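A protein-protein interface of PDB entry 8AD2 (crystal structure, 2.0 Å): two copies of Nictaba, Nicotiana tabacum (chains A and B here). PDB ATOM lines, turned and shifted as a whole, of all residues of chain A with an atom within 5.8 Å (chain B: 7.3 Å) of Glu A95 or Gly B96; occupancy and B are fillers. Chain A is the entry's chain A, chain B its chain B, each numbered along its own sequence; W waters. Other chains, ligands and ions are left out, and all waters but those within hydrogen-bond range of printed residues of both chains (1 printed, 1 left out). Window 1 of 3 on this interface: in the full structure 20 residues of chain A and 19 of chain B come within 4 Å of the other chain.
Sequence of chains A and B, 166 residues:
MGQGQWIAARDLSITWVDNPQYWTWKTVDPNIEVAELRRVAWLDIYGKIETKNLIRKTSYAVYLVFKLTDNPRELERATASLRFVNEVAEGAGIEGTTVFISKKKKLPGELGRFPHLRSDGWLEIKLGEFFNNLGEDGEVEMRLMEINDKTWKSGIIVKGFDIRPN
OG1 of Thr B98 sits at hydrogen-bond distance from OE2 of Glu A95 (2.7 Å).
The backbone NH (N) of Ala A80 sits at hydrogen-bond distance from the backbone carbonyl oxygen (O) of Thr A97 (2.8 Å).
The backbone NH of Thr B97 lies within hydrogen-bond range of the backbone carbonyl oxygen of Ala B80 (2.6 Å).
Among the printed residues, merely in contact across the chains: Glu A95 with Gly B96 (3.6 Å), Glu A95 with Thr B97 (3.5 Å), Gly A96 with Glu B95 (3.5 Å) and Thr A97 with Glu B95 (3.4 Å).
Of the printed residues of chain A, Gly B96 touches Glu A95 (3.6 Å).
Printed residues of chain A within 4 Å of Thr B98: Glu A95 (2.7 Å).
Printed residues of chain A within 4 Å of Thr B97: Glu A95 (3.5 Å).
Of the printed residues of chain B, Thr A97 touches Glu B95.
Of the printed residues of chain A, Glu B95 touches Gly A96 (3.5 Å) and Thr A97 (3.4 Å).
Printed residues of chain B within 4 Å of Gly A96: Glu B95.
Arg B83 touches none of the printed residues of chain A.
The nearest printed residue of chain B that does not touch Glu A95 is Glu B95 (5.6 Å).
The nearest residue of chain A that does not touch Gly B96 is Gly A96 (5.3 Å).
The nearest printed residue of chain A that does not touch Glu B95 is Glu A95 (5.6 Å).
Of the 9 printed residues of chain A, 3 touch a printed residue of chain B.
Among the printed residues, 5 pairs touch across the chains.
Glu A95 touches Gly B96, and with the chains exchanged Gly A96 touches Glu B95.
Glu A95 touches Thr B97, and with the chains exchanged Thr A97 touches Glu B95.
Positions printed for both chains: 80, 81, 83, 93, 94, 95, 96 and 97.
Water W1 lies within hydrogen-bond range of the backbone carbonyl oxygen of Thr B98 (2.9 Å) and the side-chain carboxylate of Glu A95 (3.2 Å).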
ATOM      1  N   ALA A  80      35.169   1.610   4.443  1.00  0.00           N
ATOM      2  CA  ALA A  80      35.137   2.649   3.430  1.00  0.00           C
ATOM      3  C   ALA A  80      33.971   3.586   3.712  1.00  0.00           C
ATOM      4  O   ALA A  80      32.897   3.188   4.193  1.00  0.00           O
ATOM      5  CB  ALA A  80      35.002   2.064   2.016  1.00  0.00           C
ATOM      6  N   SER A  81      34.177   4.849   3.380  1.00  0.00           N
ATOM      7  CA  SER A  81      33.179   5.851   3.715  1.00  0.00           C
ATOM      8  C   SER A  81      33.164   6.907   2.636  1.00  0.00           C
ATOM      9  O   SER A  81      34.225   7.270   2.123  1.00  0.00           O
ATOM     10  CB  SER A  81      33.491   6.503   5.057  1.00  0.00           C
ATOM     11  OG  SER A  81      32.863   7.792   5.141  1.00  0.00           O
ATOM     12  N   ARG A  83      30.550  10.455   1.908  1.00  0.00           N
ATOM     13  CA  ARG A  83      29.302  11.152   2.154  1.00  0.00           C
ATOM     14  C   ARG A  83      29.462  12.634   1.878  1.00  0.00           C
ATOM     15  O   ARG A  83      30.573  13.158   1.821  1.00  0.00           O
ATOM     16  CB  ARG A  83      28.850  10.908   3.578  1.00  0.00           C
ATOM     17  CG  ARG A  83      29.784  11.461   4.611  1.00  0.00           C
ATOM     18  CD  ARG A  83      29.546  10.827   5.989  1.00  0.00           C
ATOM     19  NE  ARG A  83      30.518  11.362   6.949  1.00  0.00           N
ATOM     20  CZ  ARG A  83      30.491  11.092   8.247  1.00  0.00           C
ATOM     21  NH1 ARG A  83      29.528  10.305   8.717  1.00  0.00           N
ATOM     22  NH2 ARG A  83      31.381  11.628   9.076  1.00  0.00           N
ATOM     23  N   ALA A  92      26.562  11.878  14.828  1.00  0.00           N
ATOM     24  CA  ALA A  92      26.742  10.619  14.120  1.00  0.00           C
ATOM     25  C   ALA A  92      28.229  10.341  13.910  1.00  0.00           C
ATOM     26  O   ALA A  92      29.046  11.242  13.712  1.00  0.00           O
ATOM     27  CB  ALA A  92      26.011  10.645  12.775  1.00  0.00           C
ATOM     28  N   GLY A  93      28.601   9.083  13.838  1.00  0.00           N
ATOM     29  CA  GLY A  93      29.999   8.695  13.631  1.00  0.00           C
ATOM     30  C   GLY A  93      30.344   8.639  12.157  1.00  0.00           C
ATOM     31  O   GLY A  93      29.624   9.168  11.328  1.00  0.00           O
ATOM     32  N   ILE A  94      31.391   7.928  11.802  1.00  0.00           N
ATOM     33  CA  ILE A  94      31.773   7.863  10.376  1.00  0.00           C
ATOM     34  C   ILE A  94      30.677   7.127   9.605  1.00  0.00           C
ATOM     35  O   ILE A  94      30.372   7.567   8.528  1.00  0.00           O
ATOM     36  CB  ILE A  94      33.196   7.332  10.205  1.00  0.00           C
ATOM     37  CG1 ILE A  94      34.169   8.334  10.826  1.00  0.00           C
ATOM     38  CG2 ILE A  94      33.514   7.081   8.758  1.00  0.00           C
ATOM     39  CD1 ILE A  94      34.634   7.953  12.181  1.00  0.00           C
ATOM     40  N   GLU A  95      30.081   6.098  10.189  1.00  0.00           N
ATOM     41  CA  GLU A  95      28.952   5.338   9.612  1.00  0.00           C
ATOM     42  C   GLU A  95      29.274   4.905   8.198  1.00  0.00           C
ATOM     43  O   GLU A  95      28.596   5.324   7.270  1.00  0.00           O
ATOM     44  CB  GLU A  95      27.680   6.175   9.565  1.00  0.00           C
ATOM     45  CG  GLU A  95      27.241   6.673  10.897  1.00  0.00           C
ATOM     46  CD  GLU A  95      25.907   7.363  10.830  1.00  0.00           C
ATOM     47  OE1 GLU A  95      25.682   8.161   9.917  1.00  0.00           O
ATOM     48  OE2 GLU A  95      25.098   7.127  11.703  1.00  0.00           O
ATOM     49  N   GLY A  96      30.312   4.059   7.968  1.00  0.00           N
ATOM     50  CA  GLY A  96      30.802   3.516   6.730  1.00  0.00           C
ATOM     51  C   GLY A  96      30.367   2.091   6.499  1.00  0.00           C
ATOM     52  O   GLY A  96      29.416   1.590   7.116  1.00  0.00           O
ATOM     53  N   THR A  97      31.086   1.431   5.594  1.00  0.00           N
ATOM     54  CA  THR A  97      30.717   0.125   5.081  1.00  0.00           C
ATOM     55  C   THR A  97      31.951  -0.756   4.991  1.00  0.00           C
ATOM     56  O   THR A  97      33.053  -0.280   4.706  1.00  0.00           O
ATOM     57  CB  THR A  97      30.093   0.215   3.687  1.00  0.00           C
ATOM     58  OG1 THR A  97      31.138   0.479   2.750  1.00  0.00           O
ATOM     59  CG2 THR A  97      29.066   1.308   3.607  1.00  0.00           C
ATOM     60  N   ARG B  77      15.028  10.848  14.856  1.00  0.00           N
ATOM     61  CA  ARG B  77      16.074  10.261  14.028  1.00  0.00           C
ATOM     62  C   ARG B  77      15.748   8.798  13.739  1.00  0.00           C
ATOM     63  O   ARG B  77      14.937   8.152  14.421  1.00  0.00           O
ATOM     64  CB  ARG B  77      17.479  10.292  14.685  1.00  0.00           C
ATOM     65  CG  ARG B  77      17.949  11.655  15.124  1.00  0.00           C
ATOM     66  CD  ARG B  77      19.281  11.609  15.890  1.00  0.00           C
ATOM     67  NE  ARG B  77      19.868  12.956  15.975  1.00  0.00           N
ATOM     68  CZ  ARG B  77      21.168  13.211  15.934  1.00  0.00           C
ATOM     69  NH1 ARG B  77      22.026  12.203  15.829  1.00  0.00           N
ATOM     70  NH2 ARG B  77      21.600  14.464  16.029  1.00  0.00           N
ATOM     71  N   ALA B  78      16.398   8.267  12.710  1.00  0.00           N
ATOM     72  CA  ALA B  78      16.329   6.845  12.400  1.00  0.00           C
ATOM     73  C   ALA B  78      17.516   6.530  11.504  1.00  0.00           C
ATOM     74  O   ALA B  78      18.266   7.419  11.116  1.00  0.00           O
ATOM     75  CB  ALA B  78      15.002   6.472  11.742  1.00  0.00           C
ATOM     76  N   THR B  79      17.655   5.263  11.147  1.00  0.00           N
ATOM     77  CA  THR B  79      18.758   4.754  10.356  1.00  0.00           C
ATOM     78  C   THR B  79      18.269   4.428   8.953  1.00  0.00           C
ATOM     79  O   THR B  79      17.308   3.670   8.783  1.00  0.00           O
ATOM     80  CB  THR B  79      19.354   3.513  11.018  1.00  0.00           C
ATOM     81  OG1 THR B  79      19.859   3.896  12.290  1.00  0.00           O
ATOM     82  CG2 THR B  79      20.498   2.978  10.186  1.00  0.00           C
ATOM     83  N   ALA B  80      18.930   5.000   7.953  1.00  0.00           N
ATOM     84  CA  ALA B  80      18.683   4.657   6.571  1.00  0.00           C
ATOM     85  C   ALA B  80      19.821   3.786   6.075  1.00  0.00           C
ATOM     86  O   ALA B  80      20.980   4.016   6.439  1.00  0.00           O
ATOM     87  CB  ALA B  80      18.539   5.919   5.711  1.00  0.00           C
ATOM     88  N   SER B  81      19.502   2.781   5.255  1.00  0.00           N
ATOM     89  CA  SER B  81      20.524   1.983   4.607  1.00  0.00           C
ATOM     90  C   SER B  81      20.156   1.761   3.149  1.00  0.00           C
ATOM     91  O   SER B  81      18.977   1.648   2.793  1.00  0.00           O
ATOM     92  CB  SER B  81      20.710   0.642   5.273  1.00  0.00           C
ATOM     93  OG  SER B  81      21.722  -0.076   4.573  1.00  0.00           O
ATOM     94  N   LEU B  82      21.166   1.704   2.300  1.00  0.00           N
ATOM     95  CA  LEU B  82      20.980   1.350   0.899  1.00  0.00           C
ATOM     96  C   LEU B  82      22.278   0.724   0.415  1.00  0.00           C
ATOM     97  O   LEU B  82      23.368   1.282   0.614  1.00  0.00           O
ATOM     98  CB  LEU B  82      20.622   2.569   0.015  1.00  0.00           C
ATOM     99  CG  LEU B  82      20.450   2.198  -1.452  1.00  0.00           C
ATOM    100  CD1 LEU B  82      19.352   3.029  -2.162  1.00  0.00           C
ATOM    101  CD2 LEU B  82      21.788   2.313  -2.275  1.00  0.00           C
ATOM    102  N   ARG B  83      22.165  -0.434  -0.227  1.00  0.00           N
ATOM    103  CA  ARG B  83      23.369  -1.125  -0.640  1.00  0.00           C
ATOM    104  C   ARG B  83      23.012  -2.135  -1.720  1.00  0.00           C
ATOM    105  O   ARG B  83      21.873  -2.609  -1.808  1.00  0.00           O
ATOM    106  CB  ARG B  83      24.069  -1.801   0.540  1.00  0.00           C
ATOM    107  CG  ARG B  83      23.260  -2.822   1.301  1.00  0.00           C
ATOM    108  CD  ARG B  83      23.742  -3.000   2.724  1.00  0.00           C
ATOM    109  NE  ARG B  83      23.140  -4.180   3.357  1.00  0.00           N
ATOM    110  CZ  ARG B  83      23.634  -4.772   4.442  1.00  0.00           C
ATOM    111  NH1 ARG B  83      24.737  -4.301   5.019  1.00  0.00           N
ATOM    112  NH2 ARG B  83      23.029  -5.837   4.952  1.00  0.00           N
ATOM    113  N   GLY B  93      27.079  -5.841   9.369  1.00  0.00           N
ATOM    114  CA  GLY B  93      25.690  -5.527   9.751  1.00  0.00           C
ATOM    115  C   GLY B  93      24.948  -4.765   8.666  1.00  0.00           C
ATOM    116  O   GLY B  93      25.435  -4.744   7.543  1.00  0.00           O
ATOM    117  N   ILE B  94      24.018  -3.911   9.079  1.00  0.00           N
ATOM    118  CA  ILE B  94      23.213  -3.146   8.091  1.00  0.00           C
ATOM    119  C   ILE B  94      24.048  -1.961   7.598  1.00  0.00           C
ATOM    120  O   ILE B  94      23.955  -1.640   6.410  1.00  0.00           O
ATOM    121  CB  ILE B  94      21.861  -2.722   8.695  1.00  0.00           C
ATOM    122  CG1 ILE B  94      20.981  -3.938   8.988  1.00  0.00           C
ATOM    123  CG2 ILE B  94      21.147  -1.720   7.802  1.00  0.00           C
ATOM    124  CD1 ILE B  94      19.760  -3.627   9.814  1.00  0.00           C
ATOM    125  N   GLU B  95      24.836  -1.357   8.480  1.00  0.00           N
ATOM    126  CA  GLU B  95      25.800  -0.302   8.063  1.00  0.00           C
ATOM    127  C   GLU B  95      25.043   0.837   7.368  1.00  0.00           C
ATOM    128  O   GLU B  95      25.211   0.992   6.155  1.00  0.00           O
ATOM    129  CB  GLU B  95      26.888  -0.900   7.169  1.00  0.00           C
ATOM    130  CG  GLU B  95      27.530  -2.154   7.728  1.00  0.00           C
ATOM    131  CD  GLU B  95      28.861  -2.522   7.093  1.00  0.00           C
ATOM    132  OE1 GLU B  95      28.921  -2.603   5.854  1.00  0.00           O
ATOM    133  OE2 GLU B  95      29.831  -2.725   7.841  1.00  0.00           O
ATOM    134  N   GLY B  96      24.135   1.494   8.087  1.00  0.00           N
ATOM    135  CA  GLY B  96      23.356   2.600   7.517  1.00  0.00           C
ATOM    136  C   GLY B  96      23.849   3.949   7.990  1.00  0.00           C
ATOM    137  O   GLY B  96      24.910   4.022   8.564  1.00  0.00           O
ATOM    138  N   THR B  97      23.085   4.991   7.702  1.00  0.00           N
ATOM    139  CA  THR B  97      23.377   6.360   8.068  1.00  0.00           C
ATOM    140  C   THR B  97      22.231   6.924   8.890  1.00  0.00           C
ATOM    141  O   THR B  97      21.095   6.487   8.766  1.00  0.00           O
ATOM    142  CB  THR B  97      23.602   7.192   6.820  1.00  0.00           C
ATOM    143  OG1 THR B  97      22.380   7.325   6.070  1.00  0.00           O
ATOM    144  CG2 THR B  97      24.573   6.500   5.905  1.00  0.00           C
ATOM    145  N   THR B  98      22.533   7.872   9.771  1.00  0.00           N
ATOM    146  CA  THR B  98      21.489   8.519  10.551  1.00  0.00           C
ATOM    147  C   THR B  98      20.817   9.577   9.686  1.00  0.00           C
ATOM    148  O   THR B  98      21.496  10.389   9.031  1.00  0.00           O
ATOM    149  CB  THR B  98      22.073   9.154  11.807  1.00  0.00           C
ATOM    150  OG1 THR B  98      22.758   8.145  12.539  1.00  0.00           O
ATOM    151  CG2 THR B  98      20.984   9.792  12.654  1.00  0.00           C
ATOM    152  N   VAL B  99      19.478   9.556   9.672  1.00  0.00           N
ATOM    153  CA  VAL B  99      18.670  10.579   9.016  1.00  0.00           C
ATOM    154  C   VAL B  99      17.623  11.048  10.012  1.00  0.00           C
ATOM    155  O   VAL B  99      17.380  10.406  11.036  1.00  0.00           O
ATOM    156  CB  VAL B  99      17.993  10.076   7.723  1.00  0.00           C
ATOM    157  CG1 VAL B  99      19.066   9.700   6.683  1.00  0.00           C
ATOM    158  CG2 VAL B  99      17.078   8.848   8.001  1.00  0.00           C
ATOM    159  N   LEU B 127      16.817   7.613   1.338  1.00  0.00           N
ATOM    160  CA  LEU B 127      17.475   6.506   2.000  1.00  0.00           C
ATOM    161  C   LEU B 127      18.901   6.318   1.491  1.00  0.00           C
ATOM    162  O   LEU B 127      19.774   5.871   2.234  1.00  0.00           O
ATOM    163  CB  LEU B 127      16.690   5.204   1.756  1.00  0.00           C
ATOM    164  CG  LEU B 127      15.254   5.140   2.320  1.00  0.00           C
ATOM    165  CD1 LEU B 127      14.694   3.715   2.156  1.00  0.00           C
ATOM    166  CD2 LEU B 127      15.219   5.539   3.743  1.00  0.00           C
ATOM    167  N   ARG B 143      16.370   0.293   3.484  1.00  0.00           N
ATOM    168  CA  ARG B 143      15.455   0.262   4.609  1.00  0.00           C
ATOM    169  C   ARG B 143      15.558   1.545   5.409  1.00  0.00           C
ATOM    170  O   ARG B 143      16.529   2.305   5.278  1.00  0.00           O
ATOM    171  CB  ARG B 143      15.731  -0.949   5.504  1.00  0.00           C
ATOM    172  CG  ARG B 143      17.018  -0.885   6.267  1.00  0.00           C
ATOM    173  CD  ARG B 143      17.698  -2.214   6.397  1.00  0.00           C
ATOM    174  NE  ARG B 143      16.791  -3.192   7.011  1.00  0.00           N
ATOM    175  CZ  ARG B 143      16.950  -4.498   6.902  1.00  0.00           C
ATOM    176  NH1 ARG B 143      18.001  -4.953   6.249  1.00  0.00           N
ATOM    177  NH2 ARG B 143      16.092  -5.333   7.473  1.00  0.00           N
HETATM  178  O   HOH W   1      24.317  10.971   9.338  1.00  0.00           O
